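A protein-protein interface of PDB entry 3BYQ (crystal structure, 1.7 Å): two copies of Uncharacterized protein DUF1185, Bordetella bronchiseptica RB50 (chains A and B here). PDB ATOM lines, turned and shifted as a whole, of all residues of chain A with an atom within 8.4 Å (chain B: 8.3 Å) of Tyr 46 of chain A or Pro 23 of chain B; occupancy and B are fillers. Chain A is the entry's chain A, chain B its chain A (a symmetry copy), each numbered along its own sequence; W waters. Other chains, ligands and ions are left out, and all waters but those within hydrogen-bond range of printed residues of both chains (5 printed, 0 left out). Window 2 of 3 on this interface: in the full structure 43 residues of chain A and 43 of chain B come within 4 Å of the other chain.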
ATOM      1  N   TYR A  42     -18.992 -13.364   0.947  1.00  0.00           N
ATOM      2  CA  TYR A  42     -20.124 -12.651   0.334  1.00  0.00           C
ATOM      3  C   TYR A  42     -20.487 -13.069  -1.050  1.00  0.00           C
ATOM      4  O   TYR A  42     -21.374 -12.479  -1.663  1.00  0.00           O
ATOM      5  CB  TYR A  42     -19.841 -11.149   0.357  1.00  0.00           C
ATOM      6  CG  TYR A  42     -19.464 -10.702   1.738  1.00  0.00           C
ATOM      7  CD1 TYR A  42     -20.419 -10.565   2.709  1.00  0.00           C
ATOM      8  CD2 TYR A  42     -18.152 -10.482   2.076  1.00  0.00           C
ATOM      9  CE1 TYR A  42     -20.090 -10.214   4.004  1.00  0.00           C
ATOM     10  CE2 TYR A  42     -17.808 -10.130   3.369  1.00  0.00           C
ATOM     11  CZ  TYR A  42     -18.783 -10.008   4.325  1.00  0.00           C
ATOM     12  OH  TYR A  42     -18.423  -9.654   5.623  1.00  0.00           O
ATOM     13  N   ALA A  43     -19.829 -14.121  -1.535  1.00  0.00           N
ATOM     14  CA  ALA A  43     -20.068 -14.635  -2.860  1.00  0.00           C
ATOM     15  C   ALA A  43     -21.524 -15.007  -2.971  1.00  0.00           C
ATOM     16  O   ALA A  43     -22.101 -15.621  -2.064  1.00  0.00           O
ATOM     17  CB  ALA A  43     -19.162 -15.821  -3.157  1.00  0.00           C
ATOM     18  N   GLY A  44     -22.112 -14.610  -4.084  1.00  0.00           N
ATOM     19  CA  GLY A  44     -23.499 -14.979  -4.395  1.00  0.00           C
ATOM     20  C   GLY A  44     -24.609 -14.128  -3.849  1.00  0.00           C
ATOM     21  O   GLY A  44     -25.775 -14.513  -3.916  1.00  0.00           O
ATOM     22  N   ARG A  45     -24.262 -13.029  -3.203  1.00  0.00           N
ATOM     23  CA  ARG A  45     -25.270 -12.074  -2.751  1.00  0.00           C
ATOM     24  C   ARG A  45     -24.708 -10.664  -2.631  1.00  0.00           C
ATOM     25  O   ARG A  45     -23.496 -10.441  -2.552  1.00  0.00           O
ATOM     26  CB  ARG A  45     -25.830 -12.498  -1.406  1.00  0.00           C
ATOM     27  CG  ARG A  45     -24.855 -12.278  -0.261  1.00  0.00           C
ATOM     28  CD  ARG A  45     -25.437 -12.751   1.065  1.00  0.00           C
ATOM     29  NE  ARG A  45     -24.496 -12.523   2.168  1.00  0.00           N
ATOM     30  CZ  ARG A  45     -23.428 -13.273   2.403  1.00  0.00           C
ATOM     31  NH1 ARG A  45     -23.144 -14.310   1.640  1.00  0.00           N
ATOM     32  NH2 ARG A  45     -22.652 -13.010   3.434  1.00  0.00           N
ATOM     33  N   TYR A  46     -25.620  -9.714  -2.617  1.00  0.00           N
ATOM     34  CA  TYR A  46     -25.269  -8.311  -2.428  1.00  0.00           C
ATOM     35  C   TYR A  46     -25.292  -8.008  -0.949  1.00  0.00           C
ATOM     36  O   TYR A  46     -26.347  -8.081  -0.284  1.00  0.00           O
ATOM     37  CB  TYR A  46     -26.260  -7.394  -3.133  1.00  0.00           C
ATOM     38  CG  TYR A  46     -25.927  -5.950  -2.889  1.00  0.00           C
ATOM     39  CD1 TYR A  46     -24.911  -5.331  -3.595  1.00  0.00           C
ATOM     40  CD2 TYR A  46     -26.621  -5.212  -1.939  1.00  0.00           C
ATOM     41  CE1 TYR A  46     -24.589  -4.003  -3.366  1.00  0.00           C
ATOM     42  CE2 TYR A  46     -26.306  -3.904  -1.721  1.00  0.00           C
ATOM     43  CZ  TYR A  46     -25.293  -3.309  -2.425  1.00  0.00           C
ATOM     44  OH  TYR A  46     -25.009  -1.982  -2.161  1.00  0.00           O
ATOM     45  N   GLU A  47     -24.116  -7.703  -0.423  1.00  0.00           N
ATOM     46  CA  GLU A  47     -23.960  -7.358   0.966  1.00  0.00           C
ATOM     47  C   GLU A  47     -23.728  -5.867   1.028  1.00  0.00           C
ATOM     48  O   GLU A  47     -22.725  -5.402   0.531  1.00  0.00           O
ATOM     49  CB  GLU A  47     -22.765  -8.092   1.606  1.00  0.00           C
ATOM     50  CG  GLU A  47     -22.403  -7.585   3.026  1.00  0.00           C
ATOM     51  CD  GLU A  47     -23.583  -7.538   3.967  1.00  0.00           C
ATOM     52  OE1 GLU A  47     -24.183  -8.611   4.168  1.00  0.00           O
ATOM     53  OE2 GLU A  47     -23.893  -6.433   4.509  1.00  0.00           O
ATOM     54  N   PRO A  48     -24.631  -5.102   1.667  1.00  0.00           N
ATOM     55  CA  PRO A  48     -24.434  -3.646   1.706  1.00  0.00           C
ATOM     56  C   PRO A  48     -23.250  -3.176   2.555  1.00  0.00           C
ATOM     57  O   PRO A  48     -22.644  -2.158   2.242  1.00  0.00           O
ATOM     58  CB  PRO A  48     -25.745  -3.123   2.278  1.00  0.00           C
ATOM     59  CG  PRO A  48     -26.666  -4.247   2.294  1.00  0.00           C
ATOM     60  CD  PRO A  48     -25.950  -5.498   2.198  1.00  0.00           C
ATOM     61  N   ASP A  49     -22.924  -3.930   3.597  1.00  0.00           N
ATOM     62  CA  ASP A  49     -21.851  -3.558   4.536  1.00  0.00           C
ATOM     63  C   ASP A  49     -20.629  -4.443   4.474  1.00  0.00           C
ATOM     64  O   ASP A  49     -20.556  -5.527   5.089  1.00  0.00           O
ATOM     65  CB  ASP A  49     -22.386  -3.513   5.959  1.00  0.00           C
ATOM     66  CG  ASP A  49     -21.374  -2.949   6.962  1.00  0.00           C
ATOM     67  OD1 ASP A  49     -20.344  -2.381   6.556  1.00  0.00           O
ATOM     68  OD2 ASP A  49     -21.628  -3.050   8.182  1.00  0.00           O
ATOM     69  N   LEU A  50     -19.648  -3.974   3.714  1.00  0.00           N
ATOM     70  CA  LEU A  50     -18.362  -4.694   3.527  1.00  0.00           C
ATOM     71  C   LEU A  50     -17.252  -4.148   4.439  1.00  0.00           C
ATOM     72  O   LEU A  50     -16.093  -4.578   4.368  1.00  0.00           O
ATOM     73  CB  LEU A  50     -17.940  -4.608   2.067  1.00  0.00           C
ATOM     74  CG  LEU A  50     -18.826  -5.364   1.067  1.00  0.00           C
ATOM     75  CD1 LEU A  50     -18.370  -5.073  -0.372  1.00  0.00           C
ATOM     76  CD2 LEU A  50     -18.790  -6.877   1.353  1.00  0.00           C
ATOM     77  N   ASP A  89     -18.420 -15.610  -8.821  1.00  0.00           N
ATOM     78  CA  ASP A  89     -19.654 -15.449  -8.028  1.00  0.00           C
ATOM     79  C   ASP A  89     -19.653 -14.218  -7.121  1.00  0.00           C
ATOM     80  O   ASP A  89     -20.638 -13.960  -6.453  1.00  0.00           O
ATOM     81  CB  ASP A  89     -19.982 -16.681  -7.172  1.00  0.00           C
ATOM     82  CG  ASP A  89     -20.479 -17.865  -7.986  1.00  0.00           C
ATOM     83  OD1 ASP A  89     -20.703 -17.731  -9.215  1.00  0.00           O
ATOM     84  OD2 ASP A  89     -20.672 -18.959  -7.378  1.00  0.00           O
ATOM     85  N   GLU A  91     -18.161  -9.916  -6.650  1.00  0.00           N
ATOM     86  CA  GLU A  91     -18.265  -8.605  -7.306  1.00  0.00           C
ATOM     87  C   GLU A  91     -16.981  -7.851  -7.086  1.00  0.00           C
ATOM     88  O   GLU A  91     -16.205  -8.185  -6.190  1.00  0.00           O
ATOM     89  CB  GLU A  91     -19.482  -7.818  -6.834  1.00  0.00           C
ATOM     90  CG  GLU A  91     -19.485  -7.418  -5.415  1.00  0.00           C
ATOM     91  CD  GLU A  91     -20.666  -6.510  -5.082  1.00  0.00           C
ATOM     92  OE1 GLU A  91     -20.678  -5.310  -5.485  1.00  0.00           O
ATOM     93  OE2 GLU A  91     -21.568  -6.969  -4.350  1.00  0.00           O
ATOM     94  N   GLU A  93     -16.477  -5.030  -5.836  1.00  0.00           N
ATOM     95  CA  GLU A  93     -16.350  -4.387  -4.520  1.00  0.00           C
ATOM     96  C   GLU A  93     -15.647  -5.296  -3.511  1.00  0.00           C
ATOM     97  O   GLU A  93     -15.032  -4.819  -2.559  1.00  0.00           O
ATOM     98  CB  GLU A  93     -17.700  -3.958  -3.951  1.00  0.00           C
ATOM     99  CG  GLU A  93     -17.577  -2.748  -3.040  1.00  0.00           C
ATOM    100  CD  GLU A  93     -17.237  -1.448  -3.764  1.00  0.00           C
ATOM    101  OE1 GLU A  93     -17.247  -1.419  -5.002  1.00  0.00           O
ATOM    102  OE2 GLU A  93     -17.007  -0.409  -3.089  1.00  0.00           O
ATOM    103  N   HIS A  94     -15.739  -6.596  -3.733  1.00  0.00           N
ATOM    104  CA  HIS A  94     -15.086  -7.611  -2.870  1.00  0.00           C
ATOM    105  C   HIS A  94     -13.572  -7.560  -2.986  1.00  0.00           C
ATOM    106  O   HIS A  94     -12.852  -7.982  -2.074  1.00  0.00           O
ATOM    107  CB  HIS A  94     -15.583  -9.039  -3.129  1.00  0.00           C
ATOM    108  CG  HIS A  94     -17.042  -9.223  -2.893  1.00  0.00           C
ATOM    109  ND1 HIS A  94     -17.757 -10.245  -3.489  1.00  0.00           N
ATOM    110  CD2 HIS A  94     -17.930  -8.523  -2.150  1.00  0.00           C
ATOM    111  CE1 HIS A  94     -19.012 -10.183  -3.084  1.00  0.00           C
ATOM    112  NE2 HIS A  94     -19.158  -9.123  -2.307  1.00  0.00           N
ATOM    113  N   TYR B  18     -24.239  -1.319 -16.068  1.00  0.00           N
ATOM    114  CA  TYR B  18     -25.507  -0.904 -15.459  1.00  0.00           C
ATOM    115  C   TYR B  18     -25.610  -1.314 -14.012  1.00  0.00           C
ATOM    116  O   TYR B  18     -26.189  -0.601 -13.202  1.00  0.00           O
ATOM    117  CB  TYR B  18     -26.696  -1.475 -16.219  1.00  0.00           C
ATOM    118  CG  TYR B  18     -26.754  -0.981 -17.624  1.00  0.00           C
ATOM    119  CD1 TYR B  18     -27.297   0.272 -17.907  1.00  0.00           C
ATOM    120  CD2 TYR B  18     -26.226  -1.721 -18.669  1.00  0.00           C
ATOM    121  CE1 TYR B  18     -27.331   0.756 -19.185  1.00  0.00           C
ATOM    122  CE2 TYR B  18     -26.265  -1.237 -19.969  1.00  0.00           C
ATOM    123  CZ  TYR B  18     -26.821   0.005 -20.211  1.00  0.00           C
ATOM    124  OH  TYR B  18     -26.882   0.505 -21.494  1.00  0.00           O
ATOM    125  N   HIS B  19     -25.055  -2.482 -13.711  1.00  0.00           N
ATOM    126  CA  HIS B  19     -25.038  -3.020 -12.365  1.00  0.00           C
ATOM    127  C   HIS B  19     -24.014  -4.143 -12.256  1.00  0.00           C
ATOM    128  O   HIS B  19     -23.389  -4.529 -13.247  1.00  0.00           O
ATOM    129  CB  HIS B  19     -26.415  -3.546 -11.942  1.00  0.00           C
ATOM    130  CG  HIS B  19     -26.856  -4.767 -12.690  1.00  0.00           C
ATOM    131  ND1 HIS B  19     -26.471  -6.042 -12.321  1.00  0.00           N
ATOM    132  CD2 HIS B  19     -27.651  -4.916 -13.777  1.00  0.00           C
ATOM    133  CE1 HIS B  19     -26.992  -6.918 -13.156  1.00  0.00           C
ATOM    134  NE2 HIS B  19     -27.723  -6.266 -14.041  1.00  0.00           N
ATOM    135  N   GLU B  20     -23.841  -4.613 -11.020  1.00  0.00           N
ATOM    136  CA  GLU B  20     -23.068  -5.827 -10.739  1.00  0.00           C
ATOM    137  C   GLU B  20     -23.811  -6.601  -9.664  1.00  0.00           C
ATOM    138  O   GLU B  20     -23.266  -6.951  -8.612  1.00  0.00           O
ATOM    139  CB  GLU B  20     -21.603  -5.592 -10.358  1.00  0.00           C
ATOM    140  CG  GLU B  20     -20.830  -6.867 -10.548  1.00  0.00           C
ATOM    141  CD  GLU B  20     -19.343  -6.786 -10.187  1.00  0.00           C
ATOM    142  OE1 GLU B  20     -18.858  -5.744  -9.677  1.00  0.00           O
ATOM    143  OE2 GLU B  20     -18.668  -7.770 -10.440  1.00  0.00           O
ATOM    144  N   ASN B  21     -25.094  -6.794  -9.955  1.00  0.00           N
ATOM    145  CA  ASN B  21     -26.053  -7.561  -9.169  1.00  0.00           C
ATOM    146  C   ASN B  21     -26.519  -6.943  -7.881  1.00  0.00           C
ATOM    147  O   ASN B  21     -27.191  -7.578  -7.082  1.00  0.00           O
ATOM    148  CB  ASN B  21     -25.590  -9.018  -8.988  1.00  0.00           C
ATOM    149  CG  ASN B  21     -25.308  -9.684 -10.325  1.00  0.00           C
ATOM    150  OD1 ASN B  21     -24.208 -10.173 -10.593  1.00  0.00           O
ATOM    151  ND2 ASN B  21     -26.282  -9.639 -11.190  1.00  0.00           N
ATOM    152  N   GLY B  22     -26.205  -5.674  -7.718  1.00  0.00           N
ATOM    153  CA  GLY B  22     -26.686  -4.861  -6.614  1.00  0.00           C
ATOM    154  C   GLY B  22     -27.683  -3.817  -7.135  1.00  0.00           C
ATOM    155  O   GLY B  22     -28.056  -3.847  -8.301  1.00  0.00           O
ATOM    156  N   PRO B  23     -28.116  -2.880  -6.281  1.00  0.00           N
ATOM    157  CA  PRO B  23     -29.033  -1.823  -6.721  1.00  0.00           C
ATOM    158  C   PRO B  23     -28.383  -0.955  -7.787  1.00  0.00           C
ATOM    159  O   PRO B  23     -27.324  -0.378  -7.557  1.00  0.00           O
ATOM    160  CB  PRO B  23     -29.266  -1.011  -5.449  1.00  0.00           C
ATOM    161  CG  PRO B  23     -28.947  -1.948  -4.351  1.00  0.00           C
ATOM    162  CD  PRO B  23     -27.828  -2.783  -4.843  1.00  0.00           C
ATOM    163  N   ALA B  24     -29.021  -0.873  -8.949  1.00  0.00           N
ATOM    164  CA  ALA B  24     -28.425  -0.173 -10.084  1.00  0.00           C
ATOM    165  C   ALA B  24     -28.350   1.304  -9.800  1.00  0.00           C
ATOM    166  O   ALA B  24     -29.298   1.868  -9.304  1.00  0.00           O
ATOM    167  CB  ALA B  24     -29.203  -0.407 -11.362  1.00  0.00           C
ATOM    168  N   PRO B  25     -27.217   1.934 -10.116  1.00  0.00           N
ATOM    169  CA  PRO B  25     -27.140   3.350  -9.939  1.00  0.00           C
ATOM    170  C   PRO B  25     -27.981   4.050 -10.999  1.00  0.00           C
ATOM    171  O   PRO B  25     -28.315   3.459 -12.041  1.00  0.00           O
ATOM    172  CB  PRO B  25     -25.662   3.639 -10.133  1.00  0.00           C
ATOM    173  CG  PRO B  25     -25.220   2.594 -11.058  1.00  0.00           C
ATOM    174  CD  PRO B  25     -25.937   1.385 -10.588  1.00  0.00           C
ATOM    175  N   ALA B  26     -28.291   5.300 -10.719  1.00  0.00           N
ATOM    176  CA  ALA B  26     -29.131   6.142 -11.593  1.00  0.00           C
ATOM    177  C   ALA B  26     -28.563   6.243 -12.988  1.00  0.00           C
ATOM    178  O   ALA B  26     -29.288   6.174 -13.998  1.00  0.00           O
ATOM    179  CB  ALA B  26     -29.307   7.527 -10.985  1.00  0.00           C
ATOM    180  N   ARG B 173     -17.243   3.223  -9.202  1.00  0.00           N
ATOM    181  CA  ARG B 173     -17.668   1.826  -9.359  1.00  0.00           C
ATOM    182  C   ARG B 173     -19.190   1.814  -9.153  1.00  0.00           C
ATOM    183  O   ARG B 173     -19.706   2.566  -8.316  1.00  0.00           O
ATOM    184  CB  ARG B 173     -17.026   0.925  -8.324  1.00  0.00           C
ATOM    185  CG  ARG B 173     -15.504   0.753  -8.438  1.00  0.00           C
ATOM    186  CD  ARG B 173     -14.958  -0.308  -7.459  1.00  0.00           C
ATOM    187  NE  ARG B 173     -15.253   0.087  -6.095  1.00  0.00           N
ATOM    188  CZ  ARG B 173     -14.579   1.000  -5.411  1.00  0.00           C
ATOM    189  NH1 ARG B 173     -13.561   1.640  -5.937  1.00  0.00           N
ATOM    190  NH2 ARG B 173     -14.965   1.303  -4.191  1.00  0.00           N
ATOM    191  N   VAL B 174     -19.891   0.952  -9.888  1.00  0.00           N
ATOM    192  CA  VAL B 174     -21.384   0.955  -9.844  1.00  0.00           C
ATOM    193  C   VAL B 174     -22.025   0.727  -8.452  1.00  0.00           C
ATOM    194  O   VAL B 174     -23.092   1.255  -8.168  1.00  0.00           O
ATOM    195  CB  VAL B 174     -22.020   0.043 -10.911  1.00  0.00           C
ATOM    196  CG1 VAL B 174     -21.690   0.611 -12.293  1.00  0.00           C
ATOM    197  CG2 VAL B 174     -21.592  -1.406 -10.706  1.00  0.00           C
ATOM    198  N   HIS B 175     -21.341  -0.018  -7.586  1.00  0.00           N
ATOM    199  CA  HIS B 175     -21.806  -0.240  -6.212  1.00  0.00           C
ATOM    200  C   HIS B 175     -20.756   0.159  -5.172  1.00  0.00           C
ATOM    201  O   HIS B 175     -20.656  -0.487  -4.146  1.00  0.00           O
ATOM    202  CB  HIS B 175     -22.252  -1.697  -5.981  1.00  0.00           C
ATOM    203  CG  HIS B 175     -23.233  -2.193  -6.994  1.00  0.00           C
ATOM    204  ND1 HIS B 175     -24.364  -1.490  -7.358  1.00  0.00           N
ATOM    205  CD2 HIS B 175     -23.272  -3.354  -7.687  1.00  0.00           C
ATOM    206  CE1 HIS B 175     -25.040  -2.191  -8.251  1.00  0.00           C
ATOM    207  NE2 HIS B 175     -24.395  -3.320  -8.474  1.00  0.00           N
ATOM    208  N   ALA B 176     -20.006   1.234  -5.458  1.00  0.00           N
ATOM    209  CA  ALA B 176     -18.997   1.793  -4.555  1.00  0.00           C
ATOM    210  C   ALA B 176     -19.619   2.021  -3.190  1.00  0.00           C
ATOM    211  O   ALA B 176     -20.654   2.711  -3.046  1.00  0.00           O
ATOM    212  CB  ALA B 176     -18.417   3.133  -5.115  1.00  0.00           C
ATOM    213  N   ARG B 177     -18.989   1.456  -2.162  1.00  0.00           N
ATOM    214  CA  ARG B 177     -19.542   1.559  -0.801  1.00  0.00           C
ATOM    215  C   ARG B 177     -18.552   1.301   0.301  1.00  0.00           C
ATOM    216  O   ARG B 177     -18.923   0.825   1.361  1.00  0.00           O
ATOM    217  CB  ARG B 177     -20.747   0.598  -0.631  1.00  0.00           C
ATOM    218  CG  ARG B 177     -20.483  -0.894  -0.851  1.00  0.00           C
ATOM    219  CD  ARG B 177     -21.823  -1.617  -1.032  1.00  0.00           C
ATOM    220  NE  ARG B 177     -21.728  -3.096  -1.066  1.00  0.00           N
ATOM    221  CZ  ARG B 177     -21.477  -3.817  -2.138  1.00  0.00           C
ATOM    222  NH1 ARG B 177     -21.198  -3.259  -3.297  1.00  0.00           N
ATOM    223  NH2 ARG B 177     -21.483  -5.127  -2.046  1.00  0.00           N
HETATM  224  O   HOH W   1     -19.016  -4.380  -7.302  1.00  0.00           O
HETATM  225  O   HOH W   2     -19.011  -1.737  -7.257  1.00  0.00           O
HETATM  226  O   HOH W   3     -21.849  -8.425  -2.058  1.00  0.00           O
HETATM  227  O   HOH W   4     -20.003  -1.300   2.750  1.00  0.00           O
HETATM  228  O   HOH W   5     -23.680  -7.777  -5.938  1.00  0.00           O
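No position is printed for both chains.
Of the 13 pairs that touch across the chains among the printed residues, none has its exchanged pair printed and touching as well.
Water W1 lies within hydrogen-bond range of OE1 of Glu 91 of chain A, OE1 of Glu 20 of chain B and N of Glu 93 of chain A.
Water W3 lies within hydrogen-bond range of the backbone carbonyl oxygen (O) of Arg 45 of chain A (2.6 Å), the side-chain carboxylate (OE2) of Glu 91 of chain A (2.7 Å), a ring nitrogen (NE2) of His 94 of chain A (2.8 Å), the backbone NH (N) of Glu 47 of chain A (2.9 Å) and the guanidinium group (NH2) of Arg 177 of chain B (3.3 Å).
Water W4 lies within hydrogen-bond range of O of Arg 177 of chain B (2.8 Å), O of Pro 48 of chain A (2.8 Å) and N of Leu 50 of chain A (2.9 Å).
Water W5 lies within hydrogen-bond range of the side-chain carboxylate of Glu 91 of chain A (2.8 Å) and the backbone carbonyl oxygen of Glu 20 of chain B (2.8 Å).
Water W2 bridges OE1 of Glu 93 of chain A and N of His 175 of chain B.
Tyr 46 of chain A touches three residues of chain B.
Of the printed residues of chain B, Pro 48 of chain A touches Arg 177.
Of the printed residues of chain B, Glu 91 of chain A touches Glu 20, His 175 and Arg 177.
Of chain A, only Tyr 46 comes within 4 Å of Gly 22 of chain B.
Pro 23 of chain B touches just one residue of chain A: Tyr 46 (3.5 Å).
The nearest residue of chain A that does not touch Pro 23 of chain B is Pro 48 of chain A (7.4 Å).
Among the printed residues, merely in contact across the chains: Glu 91 of chain A with Glu 20 of chain B, Glu 93 of chain A with Ala 176 of chain B, Tyr 46 of chain A with Arg 177 of chain B, Pro 48 of chain A with Arg 177 of chain B, Tyr 46 of chain A with Gly 22 of chain B, Leu 50 of chain A with Arg 177 of chain B, Tyr 46 of chain A with Pro 23 of chain B, Glu 93 of chain A with His 175 of chain B and Glu 91 of chain A with His 175 of chain B.
Of the 14 printed residues of chain B, 7 touch a printed residue of chain A.
Hydrophobic or aromatic side chains of chain B that line the printed part of chain A: Pro 23 and His 175.
Hydrophobic or aromatic side chains of chain A within 4 Å of the printed part of chain B: Tyr 46 and Leu 50.
Among the printed residues, 13 pairs touch across the chains.
Among the printed residues, Asp or Glu carboxylates within 4 Å of a Lys or Arg side-chain nitrogen of the other chain: Glu 91 of chain A with Arg 177 of chain B (3.0 Å) and Glu 93 of chain A with Arg 173 of chain B (2.7 Å).
OE1 of Glu 93 of chain A lies within salt-bridge range of NE of Arg 173 of chain B (2.7 Å).
N of Arg 177 of chain B lies within hydrogen-bond range of OE2 of Glu 93 of chain A, at 2.9 Å.
NH2 of Arg 177 of chain B lies within hydrogen-bond range of O of Glu 47 of chain A, at 2.9 Å.
OE2 of Glu 91 of chain A lies within salt-bridge range of NH2 of Arg 177 of chain B, 3.0 Å away.
N of Glu 20 of chain B sits at hydrogen-bond distance from NE2 of His 175 of chain B, at 2.9 Å.
The backbone NH (N) of Glu 91 of chain A sits at hydrogen-bond distance from a ring nitrogen (ND1) of His 94 of chain A, 3.2 Å away.
N of Asp 49 of chain A sits at hydrogen-bond distance from OE2 of Glu 47 of chain A, 2.8 Å away.
N of Gly 22 of chain B is in hydrogen-bond range of NE2 of His 175 of chain B, at 3.1 Å.
The backbone carbonyl oxygen (O) of His 175 of chain B is in hydrogen-bond range of the guanidinium group (NH1) of Arg 177 of chain B, at 2.9 Å.
The backbone carbonyl oxygen (O) of Pro 23 of chain B lies close to a ring nitrogen (ND1) of His 175 of chain B (3.2 Å).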
